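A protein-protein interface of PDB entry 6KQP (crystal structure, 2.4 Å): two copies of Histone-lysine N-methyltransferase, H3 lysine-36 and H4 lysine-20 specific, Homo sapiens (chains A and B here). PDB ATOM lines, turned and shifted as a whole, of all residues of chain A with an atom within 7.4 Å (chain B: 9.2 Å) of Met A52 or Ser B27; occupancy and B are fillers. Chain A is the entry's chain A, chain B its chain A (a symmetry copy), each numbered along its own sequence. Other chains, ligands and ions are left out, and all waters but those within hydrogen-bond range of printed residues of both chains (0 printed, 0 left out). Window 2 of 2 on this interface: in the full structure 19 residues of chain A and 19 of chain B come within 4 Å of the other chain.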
ATOM      1  N   SER A  46       7.858   8.433 -10.756  1.00  0.00           N
ATOM      2  CA  SER A  46       7.980   6.963 -10.576  1.00  0.00           C
ATOM      3  C   SER A  46       6.768   6.278 -11.209  1.00  0.00           C
ATOM      4  O   SER A  46       5.842   6.984 -11.604  1.00  0.00           O
ATOM      5  CB  SER A  46       8.099   6.584  -9.111  1.00  0.00           C
ATOM      6  OG  SER A  46       6.831   6.651  -8.471  1.00  0.00           O
ATOM      7  N   GLU A  47       6.751   4.945 -11.201  1.00  0.00           N
ATOM      8  CA  GLU A  47       5.615   4.111 -11.681  1.00  0.00           C
ATOM      9  C   GLU A  47       4.840   3.580 -10.470  1.00  0.00           C
ATOM     10  O   GLU A  47       4.180   2.548 -10.613  1.00  0.00           O
ATOM     11  CB  GLU A  47       6.134   2.943 -12.528  1.00  0.00           C
ATOM     12  CG  GLU A  47       7.184   3.332 -13.571  1.00  0.00           C
ATOM     13  CD  GLU A  47       6.749   3.302 -15.037  1.00  0.00           C
ATOM     14  OE1 GLU A  47       7.605   3.596 -15.910  1.00  0.00           O
ATOM     15  OE2 GLU A  47       5.565   2.976 -15.316  1.00  0.00           O
ATOM     16  N   CYS A  48       4.940   4.238  -9.316  1.00  0.00           N
ATOM     17  CA  CYS A  48       4.244   3.840  -8.064  1.00  0.00           C
ATOM     18  C   CYS A  48       2.758   3.599  -8.361  1.00  0.00           C
ATOM     19  O   CYS A  48       2.070   4.531  -8.843  1.00  0.00           O
ATOM     20  CB  CYS A  48       4.414   4.898  -6.985  1.00  0.00           C
ATOM     21  SG  CYS A  48       3.682   4.421  -5.403  1.00  0.00           S
ATOM     22  N   ILE A  49       2.280   2.379  -8.124  1.00  0.00           N
ATOM     23  CA  ILE A  49       0.870   2.024  -8.427  1.00  0.00           C
ATOM     24  C   ILE A  49      -0.027   2.870  -7.521  1.00  0.00           C
ATOM     25  O   ILE A  49      -1.013   3.434  -8.039  1.00  0.00           O
ATOM     26  CB  ILE A  49       0.597   0.503  -8.319  1.00  0.00           C
ATOM     27  CG1 ILE A  49      -0.840   0.156  -8.729  1.00  0.00           C
ATOM     28  CG2 ILE A  49       0.911  -0.052  -6.944  1.00  0.00           C
ATOM     29  CD1 ILE A  49      -1.210   0.594 -10.146  1.00  0.00           C
ATOM     30  N   ASN A  50       0.332   2.993  -6.229  1.00  0.00           N
ATOM     31  CA  ASN A  50      -0.416   3.822  -5.255  1.00  0.00           C
ATOM     32  C   ASN A  50      -0.551   5.232  -5.824  1.00  0.00           C
ATOM     33  O   ASN A  50      -1.690   5.758  -5.900  1.00  0.00           O
ATOM     34  CB  ASN A  50       0.259   3.850  -3.894  1.00  0.00           C
ATOM     35  CG  ASN A  50       0.200   2.501  -3.206  1.00  0.00           C
ATOM     36  OD1 ASN A  50       0.538   1.501  -3.796  1.00  0.00           O
ATOM     37  ND2 ASN A  50      -0.305   2.446  -1.994  1.00  0.00           N
ATOM     38  N   ARG A  51       0.566   5.821  -6.258  1.00  0.00           N
ATOM     39  CA  ARG A  51       0.554   7.211  -6.782  1.00  0.00           C
ATOM     40  C   ARG A  51      -0.385   7.284  -7.990  1.00  0.00           C
ATOM     41  O   ARG A  51      -1.148   8.248  -8.100  1.00  0.00           O
ATOM     42  CB  ARG A  51       1.982   7.673  -7.107  1.00  0.00           C
ATOM     43  CG  ARG A  51       2.059   9.153  -7.427  1.00  0.00           C
ATOM     44  CD  ARG A  51       3.453   9.622  -7.705  1.00  0.00           C
ATOM     45  NE  ARG A  51       4.108  10.196  -6.533  1.00  0.00           N
ATOM     46  CZ  ARG A  51       3.881  11.403  -6.036  1.00  0.00           C
ATOM     47  NH1 ARG A  51       2.952  12.183  -6.549  1.00  0.00           N
ATOM     48  NH2 ARG A  51       4.558  11.808  -4.983  1.00  0.00           N
ATOM     49  N   MET A  52      -0.349   6.286  -8.864  1.00  0.00           N
ATOM     50  CA  MET A  52      -1.119   6.322 -10.132  1.00  0.00           C
ATOM     51  C   MET A  52      -2.620   6.242  -9.843  1.00  0.00           C
ATOM     52  O   MET A  52      -3.348   6.828 -10.615  1.00  0.00           O
ATOM     53  CB  MET A  52      -0.687   5.209 -11.090  1.00  0.00           C
ATOM     54  CG  MET A  52       0.417   5.687 -12.024  1.00  0.00           C
ATOM     55  SD  MET A  52       1.094   4.407 -13.079  1.00  0.00           S
ATOM     56  CE  MET A  52       1.444   3.096 -11.911  1.00  0.00           C
ATOM     57  N   LEU A  53      -3.033   5.590  -8.751  1.00  0.00           N
ATOM     58  CA  LEU A  53      -4.455   5.496  -8.348  1.00  0.00           C
ATOM     59  C   LEU A  53      -4.851   6.651  -7.418  1.00  0.00           C
ATOM     60  O   LEU A  53      -6.014   6.599  -6.929  1.00  0.00           O
ATOM     61  CB  LEU A  53      -4.680   4.175  -7.616  1.00  0.00           C
ATOM     62  CG  LEU A  53      -4.189   2.912  -8.322  1.00  0.00           C
ATOM     63  CD1 LEU A  53      -4.711   1.684  -7.609  1.00  0.00           C
ATOM     64  CD2 LEU A  53      -4.593   2.895  -9.789  1.00  0.00           C
ATOM     65  N   LEU A  54      -3.958   7.630  -7.161  1.00  0.00           N
ATOM     66  CA  LEU A  54      -4.201   8.742  -6.193  1.00  0.00           C
ATOM     67  C   LEU A  54      -4.427   8.173  -4.791  1.00  0.00           C
ATOM     68  O   LEU A  54      -5.379   8.596  -4.064  1.00  0.00           O
ATOM     69  CB  LEU A  54      -5.411   9.571  -6.662  1.00  0.00           C
ATOM     70  CG  LEU A  54      -5.369  10.021  -8.124  1.00  0.00           C
ATOM     71  CD1 LEU A  54      -6.446  11.060  -8.412  1.00  0.00           C
ATOM     72  CD2 LEU A  54      -4.004  10.588  -8.480  1.00  0.00           C
ATOM     73  N   TYR A  55      -3.603   7.212  -4.429  1.00  0.00           N
ATOM     74  CA  TYR A  55      -3.517   6.634  -3.066  1.00  0.00           C
ATOM     75  C   TYR A  55      -2.164   7.040  -2.490  1.00  0.00           C
ATOM     76  O   TYR A  55      -1.179   7.012  -3.215  1.00  0.00           O
ATOM     77  CB  TYR A  55      -3.658   5.113  -3.125  1.00  0.00           C
ATOM     78  CG  TYR A  55      -5.084   4.649  -3.065  1.00  0.00           C
ATOM     79  CD1 TYR A  55      -5.895   4.681  -4.188  1.00  0.00           C
ATOM     80  CD2 TYR A  55      -5.630   4.198  -1.871  1.00  0.00           C
ATOM     81  CE1 TYR A  55      -7.216   4.270  -4.134  1.00  0.00           C
ATOM     82  CE2 TYR A  55      -6.949   3.788  -1.796  1.00  0.00           C
ATOM     83  CZ  TYR A  55      -7.746   3.822  -2.931  1.00  0.00           C
ATOM     84  OH  TYR A  55      -9.046   3.405  -2.862  1.00  0.00           O
ATOM     85  N   ASN A  70       5.484   9.401  -1.323  1.00  0.00           N
ATOM     86  CA  ASN A  70       4.024   9.364  -1.616  1.00  0.00           C
ATOM     87  C   ASN A  70       3.249   9.426  -0.308  1.00  0.00           C
ATOM     88  O   ASN A  70       2.431   8.527  -0.080  1.00  0.00           O
ATOM     89  CB  ASN A  70       3.636   8.115  -2.414  1.00  0.00           C
ATOM     90  CG  ASN A  70       2.244   8.185  -3.005  1.00  0.00           C
ATOM     91  OD1 ASN A  70       1.735   9.271  -3.273  1.00  0.00           O
ATOM     92  ND2 ASN A  70       1.646   7.030  -3.267  1.00  0.00           N
ATOM     93  N   TRP A 169      -7.811  12.253  -3.720  1.00  0.00           N
ATOM     94  CA  TRP A 169      -6.913  11.167  -3.278  1.00  0.00           C
ATOM     95  C   TRP A 169      -7.587  10.385  -2.170  1.00  0.00           C
ATOM     96  O   TRP A 169      -8.519  10.918  -1.597  1.00  0.00           O
ATOM     97  CB  TRP A 169      -5.585  11.718  -2.772  1.00  0.00           C
ATOM     98  CG  TRP A 169      -4.687  12.124  -3.880  1.00  0.00           C
ATOM     99  CD1 TRP A 169      -4.924  13.079  -4.816  1.00  0.00           C
ATOM    100  CD2 TRP A 169      -3.383  11.601  -4.139  1.00  0.00           C
ATOM    101  NE1 TRP A 169      -3.863  13.165  -5.669  1.00  0.00           N
ATOM    102  CE2 TRP A 169      -2.893  12.286  -5.263  1.00  0.00           C
ATOM    103  CE3 TRP A 169      -2.587  10.639  -3.520  1.00  0.00           C
ATOM    104  CZ2 TRP A 169      -1.631  12.034  -5.793  1.00  0.00           C
ATOM    105  CZ3 TRP A 169      -1.345  10.384  -4.044  1.00  0.00           C
ATOM    106  CH2 TRP A 169      -0.883  11.063  -5.177  1.00  0.00           C
ATOM    107  N   ALA B  24      -6.329   3.042 -19.701  1.00  0.00           N
ATOM    108  CA  ALA B  24      -5.200   2.634 -18.836  1.00  0.00           C
ATOM    109  C   ALA B  24      -4.384   1.565 -19.535  1.00  0.00           C
ATOM    110  O   ALA B  24      -4.968   0.695 -20.159  1.00  0.00           O
ATOM    111  CB  ALA B  24      -5.674   2.131 -17.494  1.00  0.00           C
ATOM    112  N   ASP B  25      -3.070   1.697 -19.419  1.00  0.00           N
ATOM    113  CA  ASP B  25      -2.077   0.613 -19.575  1.00  0.00           C
ATOM    114  C   ASP B  25      -2.186  -0.292 -18.345  1.00  0.00           C
ATOM    115  O   ASP B  25      -2.602   0.212 -17.266  1.00  0.00           O
ATOM    116  CB  ASP B  25      -0.682   1.224 -19.715  1.00  0.00           C
ATOM    117  CG  ASP B  25       0.308   0.298 -20.384  1.00  0.00           C
ATOM    118  OD1 ASP B  25       0.482  -0.839 -19.881  1.00  0.00           O
ATOM    119  OD2 ASP B  25       0.873   0.709 -21.415  1.00  0.00           O
ATOM    120  N   LEU B  26      -1.826  -1.570 -18.488  1.00  0.00           N
ATOM    121  CA  LEU B  26      -1.788  -2.562 -17.373  1.00  0.00           C
ATOM    122  C   LEU B  26      -0.914  -2.050 -16.232  1.00  0.00           C
ATOM    123  O   LEU B  26      -1.224  -2.385 -15.092  1.00  0.00           O
ATOM    124  CB  LEU B  26      -1.282  -3.913 -17.887  1.00  0.00           C
ATOM    125  CG  LEU B  26      -2.380  -4.938 -18.162  1.00  0.00           C
ATOM    126  CD1 LEU B  26      -3.605  -4.272 -18.788  1.00  0.00           C
ATOM    127  CD2 LEU B  26      -1.858  -6.078 -19.031  1.00  0.00           C
ATOM    128  N   SER B  27       0.115  -1.257 -16.537  1.00  0.00           N
ATOM    129  CA  SER B  27       0.969  -0.550 -15.545  1.00  0.00           C
ATOM    130  C   SER B  27       0.071   0.152 -14.530  1.00  0.00           C
ATOM    131  O   SER B  27       0.452   0.208 -13.355  1.00  0.00           O
ATOM    132  CB  SER B  27       1.890   0.478 -16.179  1.00  0.00           C
ATOM    133  OG  SER B  27       2.370   0.050 -17.444  1.00  0.00           O
ATOM    134  N   GLU B  28      -1.044   0.716 -15.002  1.00  0.00           N
ATOM    135  CA  GLU B  28      -1.866   1.700 -14.258  1.00  0.00           C
ATOM    136  C   GLU B  28      -3.048   0.987 -13.602  1.00  0.00           C
ATOM    137  O   GLU B  28      -3.872   1.680 -13.013  1.00  0.00           O
ATOM    138  CB  GLU B  28      -2.346   2.816 -15.194  1.00  0.00           C
ATOM    139  CG  GLU B  28      -1.218   3.577 -15.877  1.00  0.00           C
ATOM    140  CD  GLU B  28      -1.609   4.336 -17.139  1.00  0.00           C
ATOM    141  OE1 GLU B  28      -1.682   3.699 -18.211  1.00  0.00           O
ATOM    142  OE2 GLU B  28      -1.837   5.571 -17.051  1.00  0.00           O
ATOM    143  N   ILE B  29      -3.138  -0.338 -13.724  1.00  0.00           N
ATOM    144  CA  ILE B  29      -4.283  -1.131 -13.190  1.00  0.00           C
ATOM    145  C   ILE B  29      -3.780  -1.994 -12.042  1.00  0.00           C
ATOM    146  O   ILE B  29      -2.831  -2.765 -12.212  1.00  0.00           O
ATOM    147  CB  ILE B  29      -4.945  -1.990 -14.285  1.00  0.00           C
ATOM    148  CG1 ILE B  29      -5.313  -1.153 -15.515  1.00  0.00           C
ATOM    149  CG2 ILE B  29      -6.151  -2.728 -13.718  1.00  0.00           C
ATOM    150  CD1 ILE B  29      -6.242  -1.848 -16.509  1.00  0.00           C
ATOM    151  N   PRO B  30      -4.446  -1.940 -10.872  1.00  0.00           N
ATOM    152  CA  PRO B  30      -4.026  -2.730  -9.723  1.00  0.00           C
ATOM    153  C   PRO B  30      -4.302  -4.225  -9.900  1.00  0.00           C
ATOM    154  O   PRO B  30      -5.108  -4.614 -10.698  1.00  0.00           O
ATOM    155  CB  PRO B  30      -4.828  -2.150  -8.548  1.00  0.00           C
ATOM    156  CG  PRO B  30      -6.060  -1.563  -9.184  1.00  0.00           C
ATOM    157  CD  PRO B  30      -5.651  -1.162 -10.593  1.00  0.00           C
ATOM    158  N   ARG B  31      -3.534  -5.033  -9.192  1.00  0.00           N
ATOM    159  CA  ARG B  31      -3.645  -6.502  -9.279  1.00  0.00           C
ATOM    160  C   ARG B  31      -4.058  -7.065  -7.927  1.00  0.00           C
ATOM    161  O   ARG B  31      -3.449  -6.721  -6.940  1.00  0.00           O
ATOM    162  CB  ARG B  31      -2.301  -7.079  -9.701  1.00  0.00           C
ATOM    163  CG  ARG B  31      -2.067  -6.992 -11.195  1.00  0.00           C
ATOM    164  CD  ARG B  31      -0.587  -7.115 -11.469  1.00  0.00           C
ATOM    165  NE  ARG B  31      -0.301  -7.225 -12.886  1.00  0.00           N
ATOM    166  CZ  ARG B  31      -0.052  -6.191 -13.663  1.00  0.00           C
ATOM    167  NH1 ARG B  31      -0.057  -4.970 -13.158  1.00  0.00           N
ATOM    168  NH2 ARG B  31       0.210  -6.379 -14.942  1.00  0.00           N
ATOM    169  N   TYR B  55     -12.315  -1.013  -8.246  1.00  0.00           N
ATOM    170  CA  TYR B  55     -11.606  -1.321  -9.512  1.00  0.00           C
ATOM    171  C   TYR B  55     -12.101  -2.684  -9.983  1.00  0.00           C
ATOM    172  O   TYR B  55     -12.265  -3.573  -9.158  1.00  0.00           O
ATOM    173  CB  TYR B  55     -10.094  -1.330  -9.286  1.00  0.00           C
ATOM    174  CG  TYR B  55      -9.465   0.024  -9.443  1.00  0.00           C
ATOM    175  CD1 TYR B  55      -9.526   0.964  -8.426  1.00  0.00           C
ATOM    176  CD2 TYR B  55      -8.829   0.373 -10.626  1.00  0.00           C
ATOM    177  CE1 TYR B  55      -8.962   2.220  -8.572  1.00  0.00           C
ATOM    178  CE2 TYR B  55      -8.264   1.625 -10.793  1.00  0.00           C
ATOM    179  CZ  TYR B  55      -8.329   2.552  -9.763  1.00  0.00           C
ATOM    180  OH  TYR B  55      -7.759   3.786  -9.921  1.00  0.00           O
ATOM    181  N   HIS B  58      -8.693  -6.781 -14.142  1.00  0.00           N
ATOM    182  CA  HIS B  58      -8.526  -6.946 -15.608  1.00  0.00           C
ATOM    183  C   HIS B  58      -8.340  -8.429 -15.939  1.00  0.00           C
ATOM    184  O   HIS B  58      -7.543  -9.118 -15.298  1.00  0.00           O
ATOM    185  CB  HIS B  58      -7.373  -6.105 -16.149  1.00  0.00           C
ATOM    186  CG  HIS B  58      -7.408  -6.042 -17.634  1.00  0.00           C
ATOM    187  ND1 HIS B  58      -6.936  -7.056 -18.427  1.00  0.00           N
ATOM    188  CD2 HIS B  58      -7.932  -5.123 -18.475  1.00  0.00           C
ATOM    189  CE1 HIS B  58      -7.136  -6.748 -19.696  1.00  0.00           C
ATOM    190  NE2 HIS B  58      -7.738  -5.566 -19.751  1.00  0.00           N
ATOM    191  N   VAL B  61      -4.924 -10.455 -16.395  1.00  0.00           N
ATOM    192  CA  VAL B  61      -3.920 -10.442 -15.289  1.00  0.00           C
ATOM    193  C   VAL B  61      -4.497 -10.982 -13.984  1.00  0.00           C
ATOM    194  O   VAL B  61      -3.678 -11.289 -13.112  1.00  0.00           O
ATOM    195  CB  VAL B  61      -3.321  -9.043 -15.074  1.00  0.00           C
ATOM    196  CG1 VAL B  61      -2.287  -8.743 -16.148  1.00  0.00           C
ATOM    197  CG2 VAL B  61      -4.391  -7.954 -15.010  1.00  0.00           C
ATOM    198  N   SER B 170     -13.590   2.306 -11.366  1.00  0.00           N
ATOM    199  CA  SER B 170     -12.597   2.481 -12.460  1.00  0.00           C
ATOM    200  C   SER B 170     -12.556   1.199 -13.292  1.00  0.00           C
ATOM    201  O   SER B 170     -12.345   0.126 -12.723  1.00  0.00           O
ATOM    202  CB  SER B 170     -11.225   2.875 -11.956  1.00  0.00           C
ATOM    203  OG  SER B 170     -10.248   2.711 -12.990  1.00  0.00           O
ATOM    204  N   GLY B 173      -9.268   2.001 -16.769  1.00  0.00           N
ATOM    205  CA  GLY B 173      -8.633   3.296 -16.468  1.00  0.00           C
ATOM    206  C   GLY B 173      -9.559   4.486 -16.659  1.00  0.00           C
ATOM    207  O   GLY B 173      -9.028   5.586 -16.892  1.00  0.00           O
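Among the printed residues, merely in contact across the chains: Ile A49 with Ser B27 (3.6 Å), Ile A49 with Glu B28 (3.9 Å), Met A52 with Ser B27 (3.4 Å), Met A52 with Glu B28 (3.7 Å), Leu A53 with Glu B28 (3.5 Å), Leu A53 with Pro B30 (3.9 Å) and Leu A53 with Tyr B55 (3.3 Å).
Hydrophobic or aromatic side chains of chain B that line the printed part of chain A: Pro B30 and Tyr B55.
Of the 12 printed residues of chain A, 3 touch a printed residue of chain B.
Along chain A the printed residues that touch a printed residue of chain B span positions 49 to 53.
N of Asp B25 lies within hydrogen-bond range of OE1 of Glu B28.
OD1 of Asp B25 lies within hydrogen-bond range of OG of Ser B27 (3.2 Å).
Printed residues of chain B within 4 Å of Met A52: Ser B27 and Glu B28.
Of the printed residues of chain A, Glu B28 touches Ile A49 (3.9 Å), Met A52 (3.7 Å) and Leu A53 (3.5 Å).
Of the printed residues of chain B, Ile A49 touches Ser B27 and Glu B28.
The nearest residue of chain A that does not touch Ser B27 is Glu A47 (4.5 Å).
The nearest printed residue of chain B that does not touch Leu A53 is Ile B29 (5.3 Å).
Position printed for both chains: 55.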
